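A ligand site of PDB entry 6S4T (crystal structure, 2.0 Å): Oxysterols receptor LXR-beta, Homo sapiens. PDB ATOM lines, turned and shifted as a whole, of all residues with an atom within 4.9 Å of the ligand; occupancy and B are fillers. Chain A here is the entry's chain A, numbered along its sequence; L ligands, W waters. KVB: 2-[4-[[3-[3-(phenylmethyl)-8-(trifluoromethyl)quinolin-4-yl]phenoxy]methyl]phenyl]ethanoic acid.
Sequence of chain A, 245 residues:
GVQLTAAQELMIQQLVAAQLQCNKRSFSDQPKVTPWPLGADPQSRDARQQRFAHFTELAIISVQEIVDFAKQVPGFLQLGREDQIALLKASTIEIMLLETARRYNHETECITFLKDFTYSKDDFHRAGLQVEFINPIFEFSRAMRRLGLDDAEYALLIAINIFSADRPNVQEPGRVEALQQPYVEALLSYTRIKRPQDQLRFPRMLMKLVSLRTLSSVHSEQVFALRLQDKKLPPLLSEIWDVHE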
ATOM      1  N   ASN A  23     -15.513  26.177 -11.776  1.00  0.00           N
ATOM      2  CA  ASN A  23     -16.933  26.068 -11.529  1.00  0.00           C
ATOM      3  C   ASN A  23     -17.670  27.390 -11.755  1.00  0.00           C
ATOM      4  O   ASN A  23     -18.727  27.395 -12.379  1.00  0.00           O
ATOM      5  CB  ASN A  23     -17.236  25.577 -10.128  1.00  0.00           C
ATOM      6  CG  ASN A  23     -18.705  25.218  -9.956  1.00  0.00           C
ATOM      7  OD1 ASN A  23     -19.234  24.380 -10.686  1.00  0.00           O
ATOM      8  ND2 ASN A  23     -19.368  25.864  -9.010  1.00  0.00           N
ATOM      9  N   PHE A  27     -20.834  29.179 -15.101  1.00  0.00           N
ATOM     10  CA  PHE A  27     -21.921  30.169 -15.160  1.00  0.00           C
ATOM     11  C   PHE A  27     -21.588  31.227 -16.203  1.00  0.00           C
ATOM     12  O   PHE A  27     -22.450  31.605 -17.008  1.00  0.00           O
ATOM     13  CB  PHE A  27     -22.119  30.814 -13.792  1.00  0.00           C
ATOM     14  CG  PHE A  27     -22.572  29.854 -12.719  1.00  0.00           C
ATOM     15  CD1 PHE A  27     -21.658  28.987 -12.116  1.00  0.00           C
ATOM     16  CD2 PHE A  27     -23.905  29.808 -12.302  1.00  0.00           C
ATOM     17  CE1 PHE A  27     -22.064  28.103 -11.140  1.00  0.00           C
ATOM     18  CE2 PHE A  27     -24.310  28.914 -11.323  1.00  0.00           C
ATOM     19  CZ  PHE A  27     -23.388  28.065 -10.732  1.00  0.00           C
ATOM     20  N   PHE A  52     -34.641  14.780 -20.780  1.00  0.00           N
ATOM     21  CA  PHE A  52     -33.397  14.126 -21.189  1.00  0.00           C
ATOM     22  C   PHE A  52     -32.402  15.103 -21.834  1.00  0.00           C
ATOM     23  O   PHE A  52     -31.218  15.098 -21.507  1.00  0.00           O
ATOM     24  CB  PHE A  52     -33.701  12.969 -22.148  1.00  0.00           C
ATOM     25  CG  PHE A  52     -32.520  12.081 -22.427  1.00  0.00           C
ATOM     26  CD1 PHE A  52     -32.158  11.072 -21.533  1.00  0.00           C
ATOM     27  CD2 PHE A  52     -31.759  12.234 -23.587  1.00  0.00           C
ATOM     28  CE1 PHE A  52     -31.076  10.238 -21.793  1.00  0.00           C
ATOM     29  CE2 PHE A  52     -30.668  11.399 -23.853  1.00  0.00           C
ATOM     30  CZ  PHE A  52     -30.332  10.403 -22.946  1.00  0.00           C
ATOM     31  N   PHE A  55     -30.833  17.326 -19.311  1.00  0.00           N
ATOM     32  CA  PHE A  55     -29.791  16.570 -18.621  1.00  0.00           C
ATOM     33  C   PHE A  55     -28.520  16.380 -19.473  1.00  0.00           C
ATOM     34  O   PHE A  55     -27.419  16.533 -18.950  1.00  0.00           O
ATOM     35  CB  PHE A  55     -30.295  15.194 -18.173  1.00  0.00           C
ATOM     36  CG  PHE A  55     -31.203  15.207 -16.967  1.00  0.00           C
ATOM     37  CD1 PHE A  55     -31.269  16.289 -16.076  1.00  0.00           C
ATOM     38  CD2 PHE A  55     -31.971  14.085 -16.692  1.00  0.00           C
ATOM     39  CE1 PHE A  55     -32.104  16.241 -14.968  1.00  0.00           C
ATOM     40  CE2 PHE A  55     -32.802  14.048 -15.579  1.00  0.00           C
ATOM     41  CZ  PHE A  55     -32.875  15.121 -14.718  1.00  0.00           C
ATOM     42  N   THR A  56     -28.670  16.052 -20.756  1.00  0.00           N
ATOM     43  CA  THR A  56     -27.489  15.922 -21.635  1.00  0.00           C
ATOM     44  C   THR A  56     -26.729  17.239 -21.739  1.00  0.00           C
ATOM     45  O   THR A  56     -25.499  17.228 -21.841  1.00  0.00           O
ATOM     46  CB  THR A  56     -27.816  15.431 -23.054  1.00  0.00           C
ATOM     47  OG1 THR A  56     -28.707  16.351 -23.692  1.00  0.00           O
ATOM     48  CG2 THR A  56     -28.411  14.043 -23.031  1.00  0.00           C
ATOM     49  N   LEU A  58     -26.609  19.602 -19.294  1.00  0.00           N
ATOM     50  CA  LEU A  58     -25.866  19.675 -18.016  1.00  0.00           C
ATOM     51  C   LEU A  58     -24.588  18.840 -18.029  1.00  0.00           C
ATOM     52  O   LEU A  58     -23.553  19.303 -17.578  1.00  0.00           O
ATOM     53  CB  LEU A  58     -26.750  19.247 -16.835  1.00  0.00           C
ATOM     54  CG  LEU A  58     -27.917  20.174 -16.504  1.00  0.00           C
ATOM     55  CD1 LEU A  58     -28.764  19.575 -15.395  1.00  0.00           C
ATOM     56  CD2 LEU A  58     -27.456  21.566 -16.126  1.00  0.00           C
ATOM     57  N   ALA A  59     -24.687  17.616 -18.532  1.00  0.00           N
ATOM     58  CA  ALA A  59     -23.534  16.738 -18.684  1.00  0.00           C
ATOM     59  C   ALA A  59     -22.454  17.337 -19.582  1.00  0.00           C
ATOM     60  O   ALA A  59     -21.278  17.198 -19.274  1.00  0.00           O
ATOM     61  CB  ALA A  59     -23.966  15.389 -19.222  1.00  0.00           C
ATOM     62  N   ILE A  61     -21.987  20.629 -20.022  1.00  0.00           N
ATOM     63  CA  ILE A  61     -21.368  21.650 -19.170  1.00  0.00           C
ATOM     64  C   ILE A  61     -20.311  21.035 -18.254  1.00  0.00           C
ATOM     65  O   ILE A  61     -19.213  21.565 -18.147  1.00  0.00           O
ATOM     66  CB  ILE A  61     -22.425  22.471 -18.395  1.00  0.00           C
ATOM     67  CG1 ILE A  61     -23.054  23.499 -19.346  1.00  0.00           C
ATOM     68  CG2 ILE A  61     -21.835  23.224 -17.209  1.00  0.00           C
ATOM     69  CD1 ILE A  61     -24.475  23.841 -19.017  1.00  0.00           C
ATOM     70  N   SER A  62     -20.657  19.908 -17.628  1.00  0.00           N
ATOM     71  CA  SER A  62     -19.773  19.250 -16.657  1.00  0.00           C
ATOM     72  C   SER A  62     -18.471  18.806 -17.296  1.00  0.00           C
ATOM     73  O   SER A  62     -17.391  19.049 -16.755  1.00  0.00           O
ATOM     74  CB  SER A  62     -20.463  18.027 -16.070  1.00  0.00           C
ATOM     75  OG  SER A  62     -19.591  17.327 -15.188  1.00  0.00           O
ATOM     76  N   GLU A  65     -16.118  21.616 -17.805  1.00  0.00           N
ATOM     77  CA  GLU A  65     -15.566  22.059 -16.528  1.00  0.00           C
ATOM     78  C   GLU A  65     -14.453  21.114 -16.064  1.00  0.00           C
ATOM     79  O   GLU A  65     -13.418  21.560 -15.570  1.00  0.00           O
ATOM     80  CB  GLU A  65     -16.655  22.166 -15.451  1.00  0.00           C
ATOM     81  CG  GLU A  65     -16.174  22.748 -14.129  1.00  0.00           C
ATOM     82  CD  GLU A  65     -17.249  22.812 -13.057  1.00  0.00           C
ATOM     83  OE1 GLU A  65     -18.408  23.181 -13.375  1.00  0.00           O
ATOM     84  OE2 GLU A  65     -16.936  22.487 -11.887  1.00  0.00           O
ATOM     85  N   ILE A  93     -16.418  10.439 -16.441  1.00  0.00           N
ATOM     86  CA  ILE A  93     -17.635   9.960 -15.761  1.00  0.00           C
ATOM     87  C   ILE A  93     -17.447   9.867 -14.231  1.00  0.00           C
ATOM     88  O   ILE A  93     -18.336  10.236 -13.473  1.00  0.00           O
ATOM     89  CB  ILE A  93     -18.151   8.610 -16.320  1.00  0.00           C
ATOM     90  CG1 ILE A  93     -19.509   8.234 -15.687  1.00  0.00           C
ATOM     91  CG2 ILE A  93     -17.161   7.472 -16.091  1.00  0.00           C
ATOM     92  CD1 ILE A  93     -20.625   9.246 -15.860  1.00  0.00           C
ATOM     93  N   MET A  96     -17.415  13.368 -12.746  1.00  0.00           N
ATOM     94  CA  MET A  96     -18.787  13.835 -12.836  1.00  0.00           C
ATOM     95  C   MET A  96     -19.656  13.271 -11.713  1.00  0.00           C
ATOM     96  O   MET A  96     -20.452  14.018 -11.132  1.00  0.00           O
ATOM     97  CB  MET A  96     -19.397  13.458 -14.187  1.00  0.00           C
ATOM     98  CG  MET A  96     -20.724  14.171 -14.460  1.00  0.00           C
ATOM     99  SD  MET A  96     -21.460  13.827 -16.068  1.00  0.00           S
ATOM    100  CE  MET A  96     -20.206  14.437 -17.209  1.00  0.00           C
ATOM    101  N   LEU A  97     -19.525  11.979 -11.426  1.00  0.00           N
ATOM    102  CA  LEU A  97     -20.264  11.377 -10.313  1.00  0.00           C
ATOM    103  C   LEU A  97     -19.788  11.842  -8.931  1.00  0.00           C
ATOM    104  O   LEU A  97     -20.606  11.981  -8.019  1.00  0.00           O
ATOM    105  CB  LEU A  97     -20.279   9.851 -10.444  1.00  0.00           C
ATOM    106  CG  LEU A  97     -20.971   9.333 -11.701  1.00  0.00           C
ATOM    107  CD1 LEU A  97     -20.855   7.832 -11.777  1.00  0.00           C
ATOM    108  CD2 LEU A  97     -22.453   9.733 -11.780  1.00  0.00           C
ATOM    109  N   GLU A  99     -18.659  14.981  -8.370  1.00  0.00           N
ATOM    110  CA  GLU A  99     -19.230  16.323  -8.286  1.00  0.00           C
ATOM    111  C   GLU A  99     -20.753  16.270  -8.105  1.00  0.00           C
ATOM    112  O   GLU A  99     -21.342  17.158  -7.487  1.00  0.00           O
ATOM    113  CB  GLU A  99     -18.840  17.173  -9.514  1.00  0.00           C
ATOM    114  CG  GLU A  99     -17.360  17.576  -9.560  1.00  0.00           C
ATOM    115  CD  GLU A  99     -16.920  18.479  -8.408  1.00  0.00           C
ATOM    116  OE1 GLU A  99     -17.531  19.541  -8.204  1.00  0.00           O
ATOM    117  OE2 GLU A  99     -15.972  18.122  -7.680  1.00  0.00           O
ATOM    118  N   THR A 100     -21.376  15.211  -8.602  1.00  0.00           N
ATOM    119  CA  THR A 100     -22.786  14.947  -8.378  1.00  0.00           C
ATOM    120  C   THR A 100     -23.036  14.609  -6.907  1.00  0.00           C
ATOM    121  O   THR A 100     -23.874  15.246  -6.270  1.00  0.00           O
ATOM    122  CB  THR A 100     -23.292  13.816  -9.288  1.00  0.00           C
ATOM    123  OG1 THR A 100     -23.165  14.221 -10.666  1.00  0.00           O
ATOM    124  CG2 THR A 100     -24.747  13.489  -9.024  1.00  0.00           C
ATOM    125  N   ARG A 103     -23.128  17.418  -4.516  1.00  0.00           N
ATOM    126  CA  ARG A 103     -24.323  18.258  -4.561  1.00  0.00           C
ATOM    127  C   ARG A 103     -25.601  17.532  -4.099  1.00  0.00           C
ATOM    128  O   ARG A 103     -26.704  18.045  -4.281  1.00  0.00           O
ATOM    129  CB  ARG A 103     -24.473  18.812  -5.987  1.00  0.00           C
ATOM    130  CG  ARG A 103     -23.358  19.761  -6.387  1.00  0.00           C
ATOM    131  CD  ARG A 103     -23.217  19.912  -7.892  1.00  0.00           C
ATOM    132  NE  ARG A 103     -22.301  21.010  -8.230  1.00  0.00           N
ATOM    133  CZ  ARG A 103     -20.968  20.955  -8.170  1.00  0.00           C
ATOM    134  NH1 ARG A 103     -20.327  19.850  -7.786  1.00  0.00           N
ATOM    135  NH2 ARG A 103     -20.257  22.036  -8.492  1.00  0.00           N
ATOM    136  N   THR A 112     -28.687  19.032  -6.536  1.00  0.00           N
ATOM    137  CA  THR A 112     -28.799  20.382  -7.120  1.00  0.00           C
ATOM    138  C   THR A 112     -27.618  20.699  -8.053  1.00  0.00           C
ATOM    139  O   THR A 112     -26.480  20.736  -7.598  1.00  0.00           O
ATOM    140  CB  THR A 112     -28.896  21.462  -6.045  1.00  0.00           C
ATOM    141  OG1 THR A 112     -30.005  21.174  -5.195  1.00  0.00           O
ATOM    142  CG2 THR A 112     -29.105  22.864  -6.647  1.00  0.00           C
ATOM    143  N   PHE A 113     -27.901  20.957  -9.332  1.00  0.00           N
ATOM    144  CA  PHE A 113     -26.885  21.360 -10.327  1.00  0.00           C
ATOM    145  C   PHE A 113     -26.988  22.850 -10.657  1.00  0.00           C
ATOM    146  O   PHE A 113     -28.083  23.388 -10.892  1.00  0.00           O
ATOM    147  CB  PHE A 113     -27.046  20.570 -11.630  1.00  0.00           C
ATOM    148  CG  PHE A 113     -27.058  19.085 -11.453  1.00  0.00           C
ATOM    149  CD1 PHE A 113     -25.862  18.379 -11.322  1.00  0.00           C
ATOM    150  CD2 PHE A 113     -28.247  18.382 -11.435  1.00  0.00           C
ATOM    151  CE1 PHE A 113     -25.868  16.995 -11.161  1.00  0.00           C
ATOM    152  CE2 PHE A 113     -28.262  17.008 -11.273  1.00  0.00           C
ATOM    153  CZ  PHE A 113     -27.067  16.312 -11.145  1.00  0.00           C
ATOM    154  N   LEU A 114     -25.824  23.513 -10.667  1.00  0.00           N
ATOM    155  CA  LEU A 114     -25.703  24.943 -11.021  1.00  0.00           C
ATOM    156  C   LEU A 114     -26.598  25.869 -10.179  1.00  0.00           C
ATOM    157  O   LEU A 114     -27.095  26.880 -10.671  1.00  0.00           O
ATOM    158  CB  LEU A 114     -25.949  25.159 -12.522  1.00  0.00           C
ATOM    159  CG  LEU A 114     -25.018  24.428 -13.511  1.00  0.00           C
ATOM    160  CD1 LEU A 114     -25.500  24.666 -14.940  1.00  0.00           C
ATOM    161  CD2 LEU A 114     -23.583  24.872 -13.367  1.00  0.00           C
ATOM    162  N   PHE A 124     -35.069  11.940 -12.343  1.00  0.00           N
ATOM    163  CA  PHE A 124     -34.140  11.206 -13.217  1.00  0.00           C
ATOM    164  C   PHE A 124     -34.856  10.095 -13.972  1.00  0.00           C
ATOM    165  O   PHE A 124     -34.631   9.899 -15.175  1.00  0.00           O
ATOM    166  CB  PHE A 124     -32.957  10.626 -12.434  1.00  0.00           C
ATOM    167  CG  PHE A 124     -32.003  11.668 -11.948  1.00  0.00           C
ATOM    168  CD1 PHE A 124     -31.203  12.367 -12.850  1.00  0.00           C
ATOM    169  CD2 PHE A 124     -31.913  11.972 -10.604  1.00  0.00           C
ATOM    170  CE1 PHE A 124     -30.333  13.346 -12.410  1.00  0.00           C
ATOM    171  CE2 PHE A 124     -31.037  12.955 -10.156  1.00  0.00           C
ATOM    172  CZ  PHE A 124     -30.243  13.641 -11.062  1.00  0.00           C
ATOM    173  N   LEU A 129     -33.852   7.816 -17.564  1.00  0.00           N
ATOM    174  CA  LEU A 129     -32.728   7.066 -16.992  1.00  0.00           C
ATOM    175  C   LEU A 129     -33.261   5.935 -16.128  1.00  0.00           C
ATOM    176  O   LEU A 129     -34.304   6.081 -15.473  1.00  0.00           O
ATOM    177  CB  LEU A 129     -31.798   7.987 -16.206  1.00  0.00           C
ATOM    178  CG  LEU A 129     -31.194   9.133 -17.034  1.00  0.00           C
ATOM    179  CD1 LEU A 129     -30.616  10.214 -16.127  1.00  0.00           C
ATOM    180  CD2 LEU A 129     -30.138   8.613 -17.985  1.00  0.00           C
ATOM    181  N   PHE A 133     -29.156   2.275 -12.647  1.00  0.00           N
ATOM    182  CA  PHE A 133     -28.094   3.290 -12.661  1.00  0.00           C
ATOM    183  C   PHE A 133     -28.314   4.338 -11.568  1.00  0.00           C
ATOM    184  O   PHE A 133     -27.380   4.688 -10.845  1.00  0.00           O
ATOM    185  CB  PHE A 133     -28.054   3.951 -14.052  1.00  0.00           C
ATOM    186  CG  PHE A 133     -26.989   5.012 -14.210  1.00  0.00           C
ATOM    187  CD1 PHE A 133     -25.671   4.789 -13.801  1.00  0.00           C
ATOM    188  CD2 PHE A 133     -27.299   6.228 -14.815  1.00  0.00           C
ATOM    189  CE1 PHE A 133     -24.695   5.758 -13.967  1.00  0.00           C
ATOM    190  CE2 PHE A 133     -26.315   7.205 -14.989  1.00  0.00           C
ATOM    191  CZ  PHE A 133     -25.022   6.967 -14.558  1.00  0.00           C
ATOM    192  N   ILE A 137     -26.086   5.399  -7.812  1.00  0.00           N
ATOM    193  CA  ILE A 137     -25.600   6.788  -7.725  1.00  0.00           C
ATOM    194  C   ILE A 137     -26.026   7.441  -6.423  1.00  0.00           C
ATOM    195  O   ILE A 137     -25.222   8.121  -5.765  1.00  0.00           O
ATOM    196  CB  ILE A 137     -26.057   7.658  -8.918  1.00  0.00           C
ATOM    197  CG1 ILE A 137     -25.299   7.229 -10.172  1.00  0.00           C
ATOM    198  CG2 ILE A 137     -25.795   9.146  -8.659  1.00  0.00           C
ATOM    199  CD1 ILE A 137     -25.786   7.892 -11.443  1.00  0.00           C
ATOM    200  N   HIS A 219     -22.540   2.822 -15.535  1.00  0.00           N
ATOM    201  CA  HIS A 219     -22.868   3.897 -16.489  1.00  0.00           C
ATOM    202  C   HIS A 219     -22.795   3.424 -17.952  1.00  0.00           C
ATOM    203  O   HIS A 219     -23.661   3.771 -18.755  1.00  0.00           O
ATOM    204  CB  HIS A 219     -21.976   5.130 -16.272  1.00  0.00           C
ATOM    205  CG  HIS A 219     -22.150   6.199 -17.300  1.00  0.00           C
ATOM    206  ND1 HIS A 219     -21.284   6.374 -18.349  1.00  0.00           N
ATOM    207  CD2 HIS A 219     -23.105   7.155 -17.445  1.00  0.00           C
ATOM    208  CE1 HIS A 219     -21.684   7.380 -19.091  1.00  0.00           C
ATOM    209  NE2 HIS A 219     -22.787   7.880 -18.567  1.00  0.00           N
ATOM    210  N   GLN A 222     -26.002   1.647 -18.750  1.00  0.00           N
ATOM    211  CA  GLN A 222     -27.067   2.623 -19.007  1.00  0.00           C
ATOM    212  C   GLN A 222     -26.976   3.176 -20.441  1.00  0.00           C
ATOM    213  O   GLN A 222     -27.982   3.245 -21.135  1.00  0.00           O
ATOM    214  CB  GLN A 222     -27.009   3.768 -17.983  1.00  0.00           C
ATOM    215  CG  GLN A 222     -27.858   5.007 -18.279  1.00  0.00           C
ATOM    216  CD  GLN A 222     -29.354   4.750 -18.177  1.00  0.00           C
ATOM    217  OE1 GLN A 222     -29.984   5.108 -17.182  1.00  0.00           O
ATOM    218  NE2 GLN A 222     -29.921   4.127 -19.201  1.00  0.00           N
ATOM    219  N   VAL A 223     -25.766   3.556 -20.853  1.00  0.00           N
ATOM    220  CA  VAL A 223     -25.508   4.049 -22.211  1.00  0.00           C
ATOM    221  C   VAL A 223     -25.908   3.003 -23.261  1.00  0.00           C
ATOM    222  O   VAL A 223     -26.525   3.344 -24.276  1.00  0.00           O
ATOM    223  CB  VAL A 223     -24.020   4.446 -22.399  1.00  0.00           C
ATOM    224  CG1 VAL A 223     -23.660   4.717 -23.866  1.00  0.00           C
ATOM    225  CG2 VAL A 223     -23.694   5.690 -21.562  1.00  0.00           C
ATOM    226  N   LEU A 226     -29.715   2.636 -23.768  1.00  0.00           N
ATOM    227  CA  LEU A 226     -30.293   3.641 -24.669  1.00  0.00           C
ATOM    228  C   LEU A 226     -30.347   3.192 -26.134  1.00  0.00           C
ATOM    229  O   LEU A 226     -31.215   3.659 -26.893  1.00  0.00           O
ATOM    230  CB  LEU A 226     -29.541   4.983 -24.577  1.00  0.00           C
ATOM    231  CG  LEU A 226     -29.431   5.684 -23.219  1.00  0.00           C
ATOM    232  CD1 LEU A 226     -28.853   7.078 -23.409  1.00  0.00           C
ATOM    233  CD2 LEU A 226     -30.767   5.785 -22.492  1.00  0.00           C
ATOM    234  N   LEU A 233     -27.676   9.499 -27.264  1.00  0.00           N
ATOM    235  CA  LEU A 233     -26.904  10.625 -26.752  1.00  0.00           C
ATOM    236  C   LEU A 233     -26.551  11.594 -27.875  1.00  0.00           C
ATOM    237  O   LEU A 233     -26.392  11.173 -29.013  1.00  0.00           O
ATOM    238  CB  LEU A 233     -25.591  10.108 -26.179  1.00  0.00           C
ATOM    239  CG  LEU A 233     -25.693   9.395 -24.840  1.00  0.00           C
ATOM    240  CD1 LEU A 233     -24.472   8.519 -24.624  1.00  0.00           C
ATOM    241  CD2 LEU A 233     -25.848  10.411 -23.728  1.00  0.00           C
ATOM    242  N   TRP A 241     -18.419   8.397 -24.544  1.00  0.00           N
ATOM    243  CA  TRP A 241     -19.141   7.397 -23.731  1.00  0.00           C
ATOM    244  C   TRP A 241     -19.679   6.149 -24.451  1.00  0.00           C
ATOM    245  O   TRP A 241     -19.793   5.096 -23.829  1.00  0.00           O
ATOM    246  CB  TRP A 241     -20.269   8.061 -22.937  1.00  0.00           C
ATOM    247  CG  TRP A 241     -19.816   8.930 -21.794  1.00  0.00           C
ATOM    248  CD1 TRP A 241     -18.585   8.942 -21.177  1.00  0.00           C
ATOM    249  CD2 TRP A 241     -20.620   9.871 -21.079  1.00  0.00           C
ATOM    250  NE1 TRP A 241     -18.576   9.850 -20.157  1.00  0.00           N
ATOM    251  CE2 TRP A 241     -19.818  10.430 -20.060  1.00  0.00           C
ATOM    252  CE3 TRP A 241     -21.960  10.282 -21.180  1.00  0.00           C
ATOM    253  CZ2 TRP A 241     -20.291  11.395 -19.171  1.00  0.00           C
ATOM    254  CZ3 TRP A 241     -22.425  11.255 -20.299  1.00  0.00           C
ATOM    255  CH2 TRP A 241     -21.594  11.797 -19.306  1.00  0.00           C
HETATM  256  C7  KVB L   1     -27.587  11.380 -11.909  1.00  0.00           C
HETATM  257  C8  KVB L   1     -26.677  12.421 -11.732  1.00  0.00           C
HETATM  258  C9  KVB L   1     -25.590  12.609 -12.593  1.00  0.00           C
HETATM  259  C10 KVB L   1     -25.389  11.737 -13.664  1.00  0.00           C
HETATM  260  C11 KVB L   1     -24.223  11.945 -14.635  1.00  0.00           C
HETATM  261  C14 KVB L   1     -22.350  22.322 -11.049  1.00  0.00           C
HETATM  262  C15 KVB L   1     -21.355  21.510 -11.850  1.00  0.00           C
HETATM  263  C16 KVB L   1     -23.452  19.364 -14.155  1.00  0.00           C
HETATM  264  C19 KVB L   1     -21.708  19.041 -11.994  1.00  0.00           C
HETATM  265  C20 KVB L   1     -22.290  17.930 -12.586  1.00  0.00           C
HETATM  266  C21 KVB L   1     -23.156  18.090 -13.657  1.00  0.00           C
HETATM  267  C22 KVB L   1     -23.751  16.868 -14.262  1.00  0.00           C
HETATM  268  C24 KVB L   1     -25.311  14.885 -15.676  1.00  0.00           C
HETATM  269  C27 KVB L   1     -28.034  15.007 -15.011  1.00  0.00           C
HETATM  270  C30 KVB L   1     -26.267  12.079 -17.894  1.00  0.00           C
HETATM  271  C31 KVB L   1     -25.710  12.523 -16.647  1.00  0.00           C
HETATM  272  C32 KVB L   1     -24.809  11.647 -16.006  1.00  0.00           C
HETATM  273  C33 KVB L   1     -24.454  10.429 -16.597  1.00  0.00           C
HETATM  274  C35 KVB L   1     -25.855  10.812 -18.417  1.00  0.00           C
HETATM  275  F1  KVB L   1     -27.005   8.597 -21.106  1.00  0.00           F
HETATM  276  F2  KVB L   1     -26.122   8.088 -19.137  1.00  0.00           F
HETATM  277  F3  KVB L   1     -24.782   8.920 -20.757  1.00  0.00           F
HETATM  278  C4  KVB L   1     -26.039   9.004 -20.188  1.00  0.00           C
HETATM  279  C5  KVB L   1     -26.316  10.699 -13.831  1.00  0.00           C
HETATM  280  C6  KVB L   1     -27.403  10.511 -12.970  1.00  0.00           C
HETATM  281  O12 KVB L   1     -23.485  21.936 -10.823  1.00  0.00           O
HETATM  282  O13 KVB L   1     -21.966  23.511 -10.570  1.00  0.00           O
HETATM  283  C17 KVB L   1     -22.866  20.471 -13.576  1.00  0.00           C
HETATM  284  C18 KVB L   1     -21.999  20.301 -12.502  1.00  0.00           C
HETATM  285  O23 KVB L   1     -25.093  17.093 -14.693  1.00  0.00           O
HETATM  286  C25 KVB L   1     -25.848  16.007 -15.030  1.00  0.00           C
HETATM  287  C26 KVB L   1     -27.202  16.072 -14.716  1.00  0.00           C
HETATM  288  C28 KVB L   1     -27.517  13.882 -15.630  1.00  0.00           C
HETATM  289  C29 KVB L   1     -26.150  13.800 -15.997  1.00  0.00           C
HETATM  290  N34 KVB L   1     -24.968  10.051 -17.748  1.00  0.00           N
HETATM  291  C36 KVB L   1     -26.394  10.373 -19.654  1.00  0.00           C
HETATM  292  C37 KVB L   1     -27.324  11.149 -20.300  1.00  0.00           C
HETATM  293  C38 KVB L   1     -27.721  12.397 -19.805  1.00  0.00           C
HETATM  294  C39 KVB L   1     -27.193  12.856 -18.632  1.00  0.00           C
HETATM  295  O   HOH W   1     -23.255  24.107  -8.303  1.00  0.00           O
HETATM  296  O   HOH W   2     -18.393  19.000 -13.105  1.00  0.00           O
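NH2 of Arg 103 sits at hydrogen-bond distance from OD1 of Asn 23, at 3.4 Å.
OE1 of Glu 65 lies close to OD1 of Asn 23 (3.1 Å).
OE1 of Glu 99 is in salt-bridge range of NH1 of Arg 103, at 2.8 Å.
The backbone NH (N) of Thr 112 sits at hydrogen-bond distance from the backbone carbonyl oxygen (O) of Arg 103, at 3.2 Å.
The backbone carbonyl oxygen of Phe 124 lies within hydrogen-bond range of the backbone NH of Leu 129, at 3.3 Å.
The side-chain hydroxyl of Thr 100 sits at hydrogen-bond distance from the backbone carbonyl oxygen of Met 96, 2.8 Å away.
The backbone NH of Leu 114 sits at hydrogen-bond distance from an oxygen (O12) of the ligand (2.8 Å).
OD1 of Asn 23 lies close to O13 of the ligand (2.9 Å).
The guanidinium group (NE) of Arg 103 is in salt-bridge range of an oxygen (O12) of the ligand (3.0 Å).
N34 of the ligand is in hydrogen-bond range of NE2 of His 219 (3.2 Å).
Water W1 bridges an oxygen (O13) of the ligand (2.7 Å) and the guanidinium group (NE) of Arg 103 (3.2 Å).
Residues that only touch the ligand: Phe 55, Thr 56, Leu 58, Ala 59, Ser 62, Glu 65, Met 96, Thr 100, Phe 113, Phe 124, Phe 133, Ile 137, Gln 222, Val 223, Leu 226, Leu 233 and Trp 241.
Within 4 Å of the ligand: Asn 23, Phe 55, Thr 56, Leu 58, Ala 59, Ser 62, Glu 65, Met 96, Thr 100, Arg 103, Phe 113, Leu 114, Phe 124, Phe 133, Ile 137, His 219, Gln 222, Val 223, Leu 226, Leu 233 and Trp 241.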
